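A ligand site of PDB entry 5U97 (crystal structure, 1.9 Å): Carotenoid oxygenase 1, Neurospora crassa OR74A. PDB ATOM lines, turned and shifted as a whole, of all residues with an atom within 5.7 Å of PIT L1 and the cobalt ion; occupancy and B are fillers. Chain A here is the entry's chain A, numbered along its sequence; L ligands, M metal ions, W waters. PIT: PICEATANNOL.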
ATOM      1  N   PRO A  77       6.044 -17.633   6.104  1.00  0.00           N
ATOM      2  CA  PRO A  77       6.186 -17.111   4.750  1.00  0.00           C
ATOM      3  C   PRO A  77       7.457 -16.287   4.687  1.00  0.00           C
ATOM      4  O   PRO A  77       7.679 -15.431   5.542  1.00  0.00           O
ATOM      5  CB  PRO A  77       4.935 -16.249   4.539  1.00  0.00           C
ATOM      6  CG  PRO A  77       3.987 -16.653   5.657  1.00  0.00           C
ATOM      7  CD  PRO A  77       4.870 -17.091   6.813  1.00  0.00           C
ATOM      8  N   TRP A  90       1.508 -11.054   2.812  1.00  0.00           N
ATOM      9  CA  TRP A  90       2.331 -11.925   3.634  1.00  0.00           C
ATOM     10  C   TRP A  90       2.046 -13.396   3.352  1.00  0.00           C
ATOM     11  O   TRP A  90       2.979 -14.189   3.271  1.00  0.00           O
ATOM     12  CB  TRP A  90       2.061 -11.552   5.093  1.00  0.00           C
ATOM     13  CG  TRP A  90       2.813 -12.320   6.136  1.00  0.00           C
ATOM     14  CD1 TRP A  90       4.149 -12.560   6.216  1.00  0.00           C
ATOM     15  CD2 TRP A  90       2.217 -12.862   7.327  1.00  0.00           C
ATOM     16  NE1 TRP A  90       4.422 -13.249   7.374  1.00  0.00           N
ATOM     17  CE2 TRP A  90       3.260 -13.465   8.061  1.00  0.00           C
ATOM     18  CE3 TRP A  90       0.909 -12.911   7.820  1.00  0.00           C
ATOM     19  CZ2 TRP A  90       3.014 -14.101   9.277  1.00  0.00           C
ATOM     20  CZ3 TRP A  90       0.671 -13.571   9.013  1.00  0.00           C
ATOM     21  CH2 TRP A  90       1.722 -14.138   9.727  1.00  0.00           C
ATOM     22  N   PHE A  91       0.757 -13.743   3.137  1.00  0.00           N
ATOM     23  CA  PHE A  91       0.356 -15.128   2.934  1.00  0.00           C
ATOM     24  C   PHE A  91       0.907 -15.727   1.646  1.00  0.00           C
ATOM     25  O   PHE A  91       0.767 -16.927   1.433  1.00  0.00           O
ATOM     26  CB  PHE A  91      -1.175 -15.298   2.901  1.00  0.00           C
ATOM     27  CG  PHE A  91      -1.946 -14.910   4.126  1.00  0.00           C
ATOM     28  CD1 PHE A  91      -1.331 -14.737   5.362  1.00  0.00           C
ATOM     29  CD2 PHE A  91      -3.318 -14.677   4.042  1.00  0.00           C
ATOM     30  CE1 PHE A  91      -2.051 -14.341   6.474  1.00  0.00           C
ATOM     31  CE2 PHE A  91      -4.046 -14.260   5.155  1.00  0.00           C
ATOM     32  CZ  PHE A  91      -3.414 -14.114   6.363  1.00  0.00           C
ATOM     33  N   TYR A 133      -1.651 -13.709  -5.202  1.00  0.00           N
ATOM     34  CA  TYR A 133      -2.159 -14.724  -4.299  1.00  0.00           C
ATOM     35  C   TYR A 133      -3.355 -15.423  -4.939  1.00  0.00           C
ATOM     36  O   TYR A 133      -4.353 -14.780  -5.266  1.00  0.00           O
ATOM     37  CB  TYR A 133      -2.532 -14.083  -2.954  1.00  0.00           C
ATOM     38  CG  TYR A 133      -3.047 -15.080  -1.950  1.00  0.00           C
ATOM     39  CD1 TYR A 133      -2.194 -15.950  -1.286  1.00  0.00           C
ATOM     40  CD2 TYR A 133      -4.407 -15.229  -1.732  1.00  0.00           C
ATOM     41  CE1 TYR A 133      -2.665 -16.909  -0.396  1.00  0.00           C
ATOM     42  CE2 TYR A 133      -4.902 -16.163  -0.833  1.00  0.00           C
ATOM     43  CZ  TYR A 133      -4.025 -17.015  -0.171  1.00  0.00           C
ATOM     44  OH  TYR A 133      -4.528 -17.956   0.688  1.00  0.00           O
ATOM     45  N   ASN A 150       3.208 -22.773   3.347  1.00  0.00           N
ATOM     46  CA  ASN A 150       3.748 -21.778   4.261  1.00  0.00           C
ATOM     47  C   ASN A 150       2.901 -21.552   5.506  1.00  0.00           C
ATOM     48  O   ASN A 150       3.189 -20.628   6.257  1.00  0.00           O
ATOM     49  CB  ASN A 150       3.928 -20.446   3.542  1.00  0.00           C
ATOM     50  CG  ASN A 150       2.624 -19.778   3.167  1.00  0.00           C
ATOM     51  OD1 ASN A 150       1.544 -20.334   3.377  1.00  0.00           O
ATOM     52  ND2 ASN A 150       2.716 -18.581   2.626  1.00  0.00           N
ATOM     53  N   THR A 151       1.894 -22.392   5.769  1.00  0.00           N
ATOM     54  CA  THR A 151       0.870 -22.038   6.739  1.00  0.00           C
ATOM     55  C   THR A 151       0.953 -22.883   8.003  1.00  0.00           C
ATOM     56  O   THR A 151       0.800 -22.348   9.090  1.00  0.00           O
ATOM     57  CB  THR A 151      -0.528 -22.083   6.110  1.00  0.00           C
ATOM     58  OG1 THR A 151      -0.527 -21.192   4.991  1.00  0.00           O
ATOM     59  CG2 THR A 151      -1.620 -21.690   7.085  1.00  0.00           C
ATOM     60  N   LYS A 164      -0.779 -25.882   2.998  1.00  0.00           N
ATOM     61  CA  LYS A 164      -1.270 -24.669   2.362  1.00  0.00           C
ATOM     62  C   LYS A 164      -2.629 -24.993   1.733  1.00  0.00           C
ATOM     63  O   LYS A 164      -2.739 -25.923   0.934  1.00  0.00           O
ATOM     64  CB  LYS A 164      -0.227 -24.209   1.337  1.00  0.00           C
ATOM     65  CG  LYS A 164      -0.598 -22.987   0.521  1.00  0.00           C
ATOM     66  CD  LYS A 164      -0.868 -21.800   1.336  1.00  0.00           C
ATOM     67  CE  LYS A 164      -0.909 -20.522   0.516  1.00  0.00           C
ATOM     68  NZ  LYS A 164      -0.528 -19.378   1.365  1.00  0.00           N
ATOM     69  N   GLU A 165      -3.667 -24.237   2.089  1.00  0.00           N
ATOM     70  CA  GLU A 165      -5.059 -24.647   1.918  1.00  0.00           C
ATOM     71  C   GLU A 165      -5.519 -24.670   0.449  1.00  0.00           C
ATOM     72  O   GLU A 165      -6.638 -25.101   0.198  1.00  0.00           O
ATOM     73  CB  GLU A 165      -5.970 -23.756   2.754  1.00  0.00           C
ATOM     74  CG  GLU A 165      -6.021 -22.300   2.340  1.00  0.00           C
ATOM     75  CD  GLU A 165      -6.512 -21.372   3.431  1.00  0.00           C
ATOM     76  OE1 GLU A 165      -7.506 -20.604   3.188  1.00  0.00           O
ATOM     77  OE2 GLU A 165      -5.923 -21.419   4.547  1.00  0.00           O
ATOM     78  N   ALA A 196      -4.936 -26.312   6.180  1.00  0.00           N
ATOM     79  CA  ALA A 196      -3.807 -26.068   7.046  1.00  0.00           C
ATOM     80  C   ALA A 196      -4.112 -26.479   8.487  1.00  0.00           C
ATOM     81  O   ALA A 196      -3.217 -26.419   9.327  1.00  0.00           O
ATOM     82  CB  ALA A 196      -3.409 -24.616   6.967  1.00  0.00           C
ATOM     83  N   HIS A 197      -5.346 -26.900   8.798  1.00  0.00           N
ATOM     84  CA  HIS A 197      -5.742 -27.158  10.175  1.00  0.00           C
ATOM     85  C   HIS A 197      -6.421 -28.518  10.331  1.00  0.00           C
ATOM     86  O   HIS A 197      -7.523 -28.604  10.854  1.00  0.00           O
ATOM     87  CB  HIS A 197      -6.605 -26.008  10.694  1.00  0.00           C
ATOM     88  CG  HIS A 197      -5.814 -24.773  10.910  1.00  0.00           C
ATOM     89  ND1 HIS A 197      -4.907 -24.694  11.942  1.00  0.00           N
ATOM     90  CD2 HIS A 197      -5.760 -23.589  10.266  1.00  0.00           C
ATOM     91  CE1 HIS A 197      -4.321 -23.508  11.915  1.00  0.00           C
ATOM     92  NE2 HIS A 197      -4.829 -22.812  10.900  1.00  0.00           N
ATOM     93  N   MET A 246     -13.992 -18.608   2.109  1.00  0.00           N
ATOM     94  CA  MET A 246     -12.763 -19.111   2.701  1.00  0.00           C
ATOM     95  C   MET A 246     -13.087 -19.870   3.989  1.00  0.00           C
ATOM     96  O   MET A 246     -13.675 -19.315   4.911  1.00  0.00           O
ATOM     97  CB  MET A 246     -11.795 -17.964   2.999  1.00  0.00           C
ATOM     98  CG  MET A 246     -10.530 -18.409   3.723  1.00  0.00           C
ATOM     99  SD  MET A 246      -9.518 -17.044   4.331  1.00  0.00           S
ATOM    100  CE  MET A 246      -8.831 -16.402   2.809  1.00  0.00           C
ATOM    101  N   HIS A 248     -10.831 -21.381   6.531  1.00  0.00           N
ATOM    102  CA  HIS A 248      -9.434 -21.482   6.944  1.00  0.00           C
ATOM    103  C   HIS A 248      -9.227 -22.580   7.989  1.00  0.00           C
ATOM    104  O   HIS A 248      -8.227 -23.311   7.959  1.00  0.00           O
ATOM    105  CB  HIS A 248      -8.911 -20.142   7.462  1.00  0.00           C
ATOM    106  CG  HIS A 248      -7.489 -20.260   7.910  1.00  0.00           C
ATOM    107  ND1 HIS A 248      -6.482 -20.519   7.014  1.00  0.00           N
ATOM    108  CD2 HIS A 248      -6.928 -20.236   9.132  1.00  0.00           C
ATOM    109  CE1 HIS A 248      -5.329 -20.626   7.676  1.00  0.00           C
ATOM    110  NE2 HIS A 248      -5.580 -20.456   8.960  1.00  0.00           N
ATOM    111  N   ASP A 249     -10.160 -22.676   8.944  1.00  0.00           N
ATOM    112  CA  ASP A 249     -10.052 -23.610  10.051  1.00  0.00           C
ATOM    113  C   ASP A 249     -11.364 -24.373  10.147  1.00  0.00           C
ATOM    114  O   ASP A 249     -12.338 -23.996   9.506  1.00  0.00           O
ATOM    115  CB  ASP A 249      -9.669 -22.846  11.329  1.00  0.00           C
ATOM    116  CG  ASP A 249      -9.062 -23.688  12.447  1.00  0.00           C
ATOM    117  OD1 ASP A 249      -9.072 -24.939  12.324  1.00  0.00           O
ATOM    118  OD2 ASP A 249      -8.586 -23.074  13.422  1.00  0.00           O
ATOM    119  N   PHE A 310     -16.017 -12.455  11.143  1.00  0.00           N
ATOM    120  CA  PHE A 310     -14.834 -13.164  10.670  1.00  0.00           C
ATOM    121  C   PHE A 310     -14.620 -14.416  11.518  1.00  0.00           C
ATOM    122  O   PHE A 310     -14.494 -14.326  12.736  1.00  0.00           O
ATOM    123  CB  PHE A 310     -13.637 -12.223  10.718  1.00  0.00           C
ATOM    124  CG  PHE A 310     -12.389 -12.763  10.074  1.00  0.00           C
ATOM    125  CD1 PHE A 310     -11.545 -13.617  10.762  1.00  0.00           C
ATOM    126  CD2 PHE A 310     -12.081 -12.455   8.755  1.00  0.00           C
ATOM    127  CE1 PHE A 310     -10.408 -14.128  10.156  1.00  0.00           C
ATOM    128  CE2 PHE A 310     -10.944 -12.967   8.149  1.00  0.00           C
ATOM    129  CZ  PHE A 310     -10.113 -13.807   8.852  1.00  0.00           C
ATOM    130  N   ALA A 311     -14.576 -15.584  10.862  1.00  0.00           N
ATOM    131  CA  ALA A 311     -14.256 -16.845  11.528  1.00  0.00           C
ATOM    132  C   ALA A 311     -12.746 -16.952  11.724  1.00  0.00           C
ATOM    133  O   ALA A 311     -12.022 -17.317  10.806  1.00  0.00           O
ATOM    134  CB  ALA A 311     -14.781 -18.009  10.715  1.00  0.00           C
ATOM    135  N   GLY A 312     -12.289 -16.613  12.937  1.00  0.00           N
ATOM    136  CA  GLY A 312     -10.893 -16.789  13.326  1.00  0.00           C
ATOM    137  C   GLY A 312     -10.594 -18.244  13.724  1.00  0.00           C
ATOM    138  O   GLY A 312     -11.401 -19.130  13.510  1.00  0.00           O
ATOM    139  N   HIS A 313      -9.419 -18.477  14.311  1.00  0.00           N
ATOM    140  CA  HIS A 313      -8.947 -19.814  14.605  1.00  0.00           C
ATOM    141  C   HIS A 313      -9.793 -20.479  15.682  1.00  0.00           C
ATOM    142  O   HIS A 313     -10.239 -19.832  16.639  1.00  0.00           O
ATOM    143  CB  HIS A 313      -7.471 -19.800  15.024  1.00  0.00           C
ATOM    144  CG  HIS A 313      -6.540 -19.622  13.883  1.00  0.00           C
ATOM    145  ND1 HIS A 313      -5.831 -18.461  13.646  1.00  0.00           N
ATOM    146  CD2 HIS A 313      -6.228 -20.453  12.898  1.00  0.00           C
ATOM    147  CE1 HIS A 313      -5.094 -18.631  12.557  1.00  0.00           C
ATOM    148  NE2 HIS A 313      -5.325 -19.822  12.087  1.00  0.00           N
ATOM    149  N   VAL A 336     -10.905  -9.037   9.071  1.00  0.00           N
ATOM    150  CA  VAL A 336      -9.554  -9.026   9.583  1.00  0.00           C
ATOM    151  C   VAL A 336      -8.557  -8.909   8.417  1.00  0.00           C
ATOM    152  O   VAL A 336      -7.512  -8.282   8.571  1.00  0.00           O
ATOM    153  CB  VAL A 336      -9.301 -10.279  10.446  1.00  0.00           C
ATOM    154  CG1 VAL A 336      -7.839 -10.420  10.844  1.00  0.00           C
ATOM    155  CG2 VAL A 336     -10.211 -10.294  11.669  1.00  0.00           C
ATOM    156  N   PHE A 337      -8.898  -9.505   7.267  1.00  0.00           N
ATOM    157  CA  PHE A 337      -8.060  -9.425   6.081  1.00  0.00           C
ATOM    158  C   PHE A 337      -8.485  -8.211   5.247  1.00  0.00           C
ATOM    159  O   PHE A 337      -9.011  -8.332   4.141  1.00  0.00           O
ATOM    160  CB  PHE A 337      -8.119 -10.745   5.301  1.00  0.00           C
ATOM    161  CG  PHE A 337      -7.693 -11.984   6.049  1.00  0.00           C
ATOM    162  CD1 PHE A 337      -7.019 -11.913   7.257  1.00  0.00           C
ATOM    163  CD2 PHE A 337      -8.011 -13.240   5.559  1.00  0.00           C
ATOM    164  CE1 PHE A 337      -6.654 -13.065   7.935  1.00  0.00           C
ATOM    165  CE2 PHE A 337      -7.646 -14.392   6.237  1.00  0.00           C
ATOM    166  CZ  PHE A 337      -6.956 -14.306   7.425  1.00  0.00           C
ATOM    167  N   GLU A 383      -6.023 -14.070  19.482  1.00  0.00           N
ATOM    168  CA  GLU A 383      -6.002 -14.995  18.355  1.00  0.00           C
ATOM    169  C   GLU A 383      -5.016 -16.130  18.653  1.00  0.00           C
ATOM    170  O   GLU A 383      -4.400 -16.167  19.722  1.00  0.00           O
ATOM    171  CB  GLU A 383      -5.685 -14.271  17.040  1.00  0.00           C
ATOM    172  CG  GLU A 383      -6.852 -14.225  16.049  1.00  0.00           C
ATOM    173  CD  GLU A 383      -7.161 -15.514  15.293  1.00  0.00           C
ATOM    174  OE1 GLU A 383      -6.519 -16.558  15.553  1.00  0.00           O
ATOM    175  OE2 GLU A 383      -8.073 -15.475  14.428  1.00  0.00           O
ATOM    176  N   PHE A 384      -4.918 -17.076  17.703  1.00  0.00           N
ATOM    177  CA  PHE A 384      -3.942 -18.161  17.734  1.00  0.00           C
ATOM    178  C   PHE A 384      -4.083 -18.981  19.010  1.00  0.00           C
ATOM    179  O   PHE A 384      -3.110 -19.192  19.733  1.00  0.00           O
ATOM    180  CB  PHE A 384      -2.538 -17.595  17.549  1.00  0.00           C
ATOM    181  CG  PHE A 384      -2.437 -16.605  16.417  1.00  0.00           C
ATOM    182  CD1 PHE A 384      -2.094 -15.288  16.666  1.00  0.00           C
ATOM    183  CD2 PHE A 384      -2.741 -16.984  15.115  1.00  0.00           C
ATOM    184  CE1 PHE A 384      -2.030 -14.371  15.626  1.00  0.00           C
ATOM    185  CE2 PHE A 384      -2.683 -16.065  14.088  1.00  0.00           C
ATOM    186  CZ  PHE A 384      -2.328 -14.768  14.345  1.00  0.00           C
ATOM    187  N   PRO A 425      -0.007  -9.821  11.653  1.00  0.00           N
ATOM    188  CA  PRO A 425      -0.712  -9.439  12.881  1.00  0.00           C
ATOM    189  C   PRO A 425       0.278  -9.248  14.029  1.00  0.00           C
ATOM    190  O   PRO A 425       1.363  -9.806  13.995  1.00  0.00           O
ATOM    191  CB  PRO A 425      -1.636 -10.620  13.165  1.00  0.00           C
ATOM    192  CG  PRO A 425      -0.888 -11.792  12.569  1.00  0.00           C
ATOM    193  CD  PRO A 425      -0.210 -11.245  11.339  1.00  0.00           C
ATOM    194  N   LEU A 509       3.578 -18.241  10.757  1.00  0.00           N
ATOM    195  CA  LEU A 509       2.233 -18.737  10.973  1.00  0.00           C
ATOM    196  C   LEU A 509       2.304 -19.841  12.015  1.00  0.00           C
ATOM    197  O   LEU A 509       2.781 -19.571  13.127  1.00  0.00           O
ATOM    198  CB  LEU A 509       1.635 -19.116   9.608  1.00  0.00           C
ATOM    199  CG  LEU A 509       1.292 -17.919   8.716  1.00  0.00           C
ATOM    200  CD1 LEU A 509       0.970 -18.346   7.294  1.00  0.00           C
ATOM    201  CD2 LEU A 509       0.138 -17.134   9.300  1.00  0.00           C
ATOM    202  N   HIS A 510       1.915 -21.065  11.677  1.00  0.00           N
ATOM    203  CA  HIS A 510       1.650 -22.076  12.700  1.00  0.00           C
ATOM    204  C   HIS A 510       2.887 -22.912  12.992  1.00  0.00           C
ATOM    205  O   HIS A 510       3.834 -22.965  12.202  1.00  0.00           O
ATOM    206  CB  HIS A 510       0.429 -22.916  12.308  1.00  0.00           C
ATOM    207  CG  HIS A 510      -0.819 -22.106  12.224  1.00  0.00           C
ATOM    208  ND1 HIS A 510      -1.453 -21.607  13.340  1.00  0.00           N
ATOM    209  CD2 HIS A 510      -1.557 -21.709  11.160  1.00  0.00           C
ATOM    210  CE1 HIS A 510      -2.524 -20.915  12.953  1.00  0.00           C
ATOM    211  NE2 HIS A 510      -2.612 -20.973  11.637  1.00  0.00           N
HETATM  212  C1  PIT L   1      -6.567 -15.944  11.328  1.00  0.00           C
HETATM  213  C2  PIT L   1      -5.835 -14.944  11.951  1.00  0.00           C
HETATM  214  C3  PIT L   1      -4.610 -14.567  11.417  1.00  0.00           C
HETATM  215  C4  PIT L   1      -4.118 -15.197  10.282  1.00  0.00           C
HETATM  216  C5  PIT L   1      -4.857 -16.179   9.636  1.00  0.00           C
HETATM  217  C6  PIT L   1      -6.095 -16.555  10.166  1.00  0.00           C
HETATM  218  C7  PIT L   1      -4.258 -16.761   8.424  1.00  0.00           C
HETATM  219  C8  PIT L   1      -4.877 -17.364   7.426  1.00  0.00           C
HETATM  220  C9  PIT L   1      -4.287 -17.791   6.157  1.00  0.00           C
HETATM  221  C10 PIT L   1      -2.901 -17.921   5.935  1.00  0.00           C
HETATM  222  C11 PIT L   1      -2.403 -18.304   4.692  1.00  0.00           C
HETATM  223  C12 PIT L   1      -3.290 -18.512   3.632  1.00  0.00           C
HETATM  224  C13 PIT L   1      -4.651 -18.359   3.827  1.00  0.00           C
HETATM  225  C14 PIT L   1      -5.128 -17.988   5.073  1.00  0.00           C
HETATM  226  O1  PIT L   1      -2.871 -18.878   2.379  1.00  0.00           O
HETATM  227  O2  PIT L   1      -3.817 -13.590  11.937  1.00  0.00           O
HETATM  228  O3  PIT L   1      -7.808 -16.314  11.825  1.00  0.00           O
HETATM  229  OAD PIT L   1      -1.042 -18.475   4.454  1.00  0.00           O
HETATM  230  C1  PIT L   2       0.422  -3.025  10.181  1.00  0.00           C
HETATM  231  C2  PIT L   2       0.743  -2.284   9.041  1.00  0.00           C
HETATM  232  C3  PIT L   2       0.279  -2.708   7.796  1.00  0.00           C
HETATM  233  C4  PIT L   2      -0.483  -3.867   7.691  1.00  0.00           C
HETATM  234  C5  PIT L   2      -0.832  -4.585   8.831  1.00  0.00           C
HETATM  235  C6  PIT L   2      -0.352  -4.183  10.071  1.00  0.00           C
HETATM  236  C7  PIT L   2      -1.626  -5.818   8.683  1.00  0.00           C
HETATM  237  C8  PIT L   2      -2.258  -6.475   9.638  1.00  0.00           C
HETATM  238  C9  PIT L   2      -2.642  -7.889   9.585  1.00  0.00           C
HETATM  239  C10 PIT L   2      -3.555  -8.442  10.492  1.00  0.00           C
HETATM  240  C11 PIT L   2      -3.886  -9.782  10.429  1.00  0.00           C
HETATM  241  C12 PIT L   2      -3.278 -10.607   9.483  1.00  0.00           C
HETATM  242  C13 PIT L   2      -2.360 -10.081   8.598  1.00  0.00           C
HETATM  243  C14 PIT L   2      -2.051  -8.740   8.661  1.00  0.00           C
HETATM  244  O1  PIT L   2      -3.564 -11.955   9.399  1.00  0.00           O
HETATM  245  O2  PIT L   2       0.563  -2.016   6.645  1.00  0.00           O
HETATM  246  O3  PIT L   2       0.856  -2.639  11.422  1.00  0.00           O
HETATM  247  OAD PIT L   2      -4.789 -10.299  11.317  1.00  0.00           O
HETATM  248 CO    CO M   1      -4.403 -20.809  10.591  1.00  0.00          CO
HETATM  249  O   HOH W   1      -2.989 -19.079   9.474  1.00  0.00           O
HETATM  250  O   HOH W   2      -9.477 -18.376  10.690  1.00  0.00           O
HETATM  251  O   HOH W   3      -5.057 -11.987  13.768  1.00  0.00           O
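A ring nitrogen (ND1) of His 313 lies within hydrogen-bond range of the side-chain carboxylate (OE1) of Glu 383 (2.8 Å).
ND1 of His 248 is in hydrogen-bond range of OE2 of Glu 165, at 2.7 Å.
O of Thr 151 sits at hydrogen-bond distance from N of His 510 (3.1 Å).
The side-chain amide oxygen of Asn 150 lies within hydrogen-bond range of the side-chain amino group of Lys 164.
NZ of Lys 164 is in hydrogen-bond range of O of Phe 91 (2.8 Å).
OD1 of Asn 150 is in hydrogen-bond range of OG1 of Thr 151, at 2.8 Å.
ND2 of Asn 150 lies within hydrogen-bond range of O of Phe 91 (2.8 Å).
An oxygen (O2) of PIT L1 sits at hydrogen-bond distance from an oxygen (O1) of PIT L2, at 3.0 Å.
A ring nitrogen (ND1) of His 313 sits at hydrogen-bond distance from an oxygen (O3) of PIT L1 (3.4 Å).
The side-chain hydroxyl (OH) of Tyr 133 sits at hydrogen-bond distance from an oxygen (O1) of PIT L1, 2.5 Å away.
O1 of PIT L1 sits at hydrogen-bond distance from NZ of Lys 164, at 2.6 Å.
An oxygen (O3) of PIT L1 sits at hydrogen-bond distance from the side-chain carboxylate (OE2) of Glu 383 (2.7 Å).
OG1 of Thr 151 sits at hydrogen-bond distance from OAD of PIT L1 (2.8 Å).
An oxygen (OAD) of PIT L1 lies within hydrogen-bond range of the side-chain amide oxygen (OD1) of Asn 150, 3.4 Å away.
The cobalt ion is bound by a ring nitrogen (NE2) of His 313 (2.0 Å), a ring nitrogen (NE2) of His 248 (2.0 Å), a ring nitrogen (NE2) of His 197 (2.1 Å), a ring nitrogen (NE2) of His 510 (2.1 Å) and water W1 (2.5 Å).
The cobalt ion has five donor atoms within binding distance.
CZ of Phe 91 touches C7 of PIT L1 (3.5 Å).
Glu 165 touches PIT L1 (OE2 to C13, 3.4 Å).
CE1 of Phe 310 touches O3 of PIT L1, at 3.8 Å.
Gly 312 touches PIT L1 (CA to O3, 3.5 Å).
Phe 337 touches PIT L1.
CZ of Phe 384 touches O2 of PIT L1, at 3.1 Å.
Pro 425 touches PIT L1.
CD1 of Leu 509 touches OAD of PIT L1, at 3.5 Å.
Hydrophobic or aromatic side chains within 4 Å of PIT L1: Phe 91, Tyr 133, His 248, Phe 310, His 313, Phe 337, Phe 384, Pro 425 and Leu 509.
The nearest printed residue that does not touch PIT L1 is Ala 311 (4.4 Å).
Of the 24 residues printed, 4 come within 4 Å of the cobalt ion.
Along chain A the residues within 4 Å of the cobalt ion span positions 197 to 510.
The nearest printed residue that does not touch the cobalt ion is Thr 151 (4.6 Å).
Water W3 lies within hydrogen-bond range of an oxygen (O2) of PIT L1 (2.7 Å) and an oxygen (OAD) of PIT L2 (3.0 Å).
Water W2 lies within hydrogen-bond range of O of Ala 311 (2.8 Å), O3 of PIT L1 (2.9 Å) and O of Gly 312 (3.5 Å).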
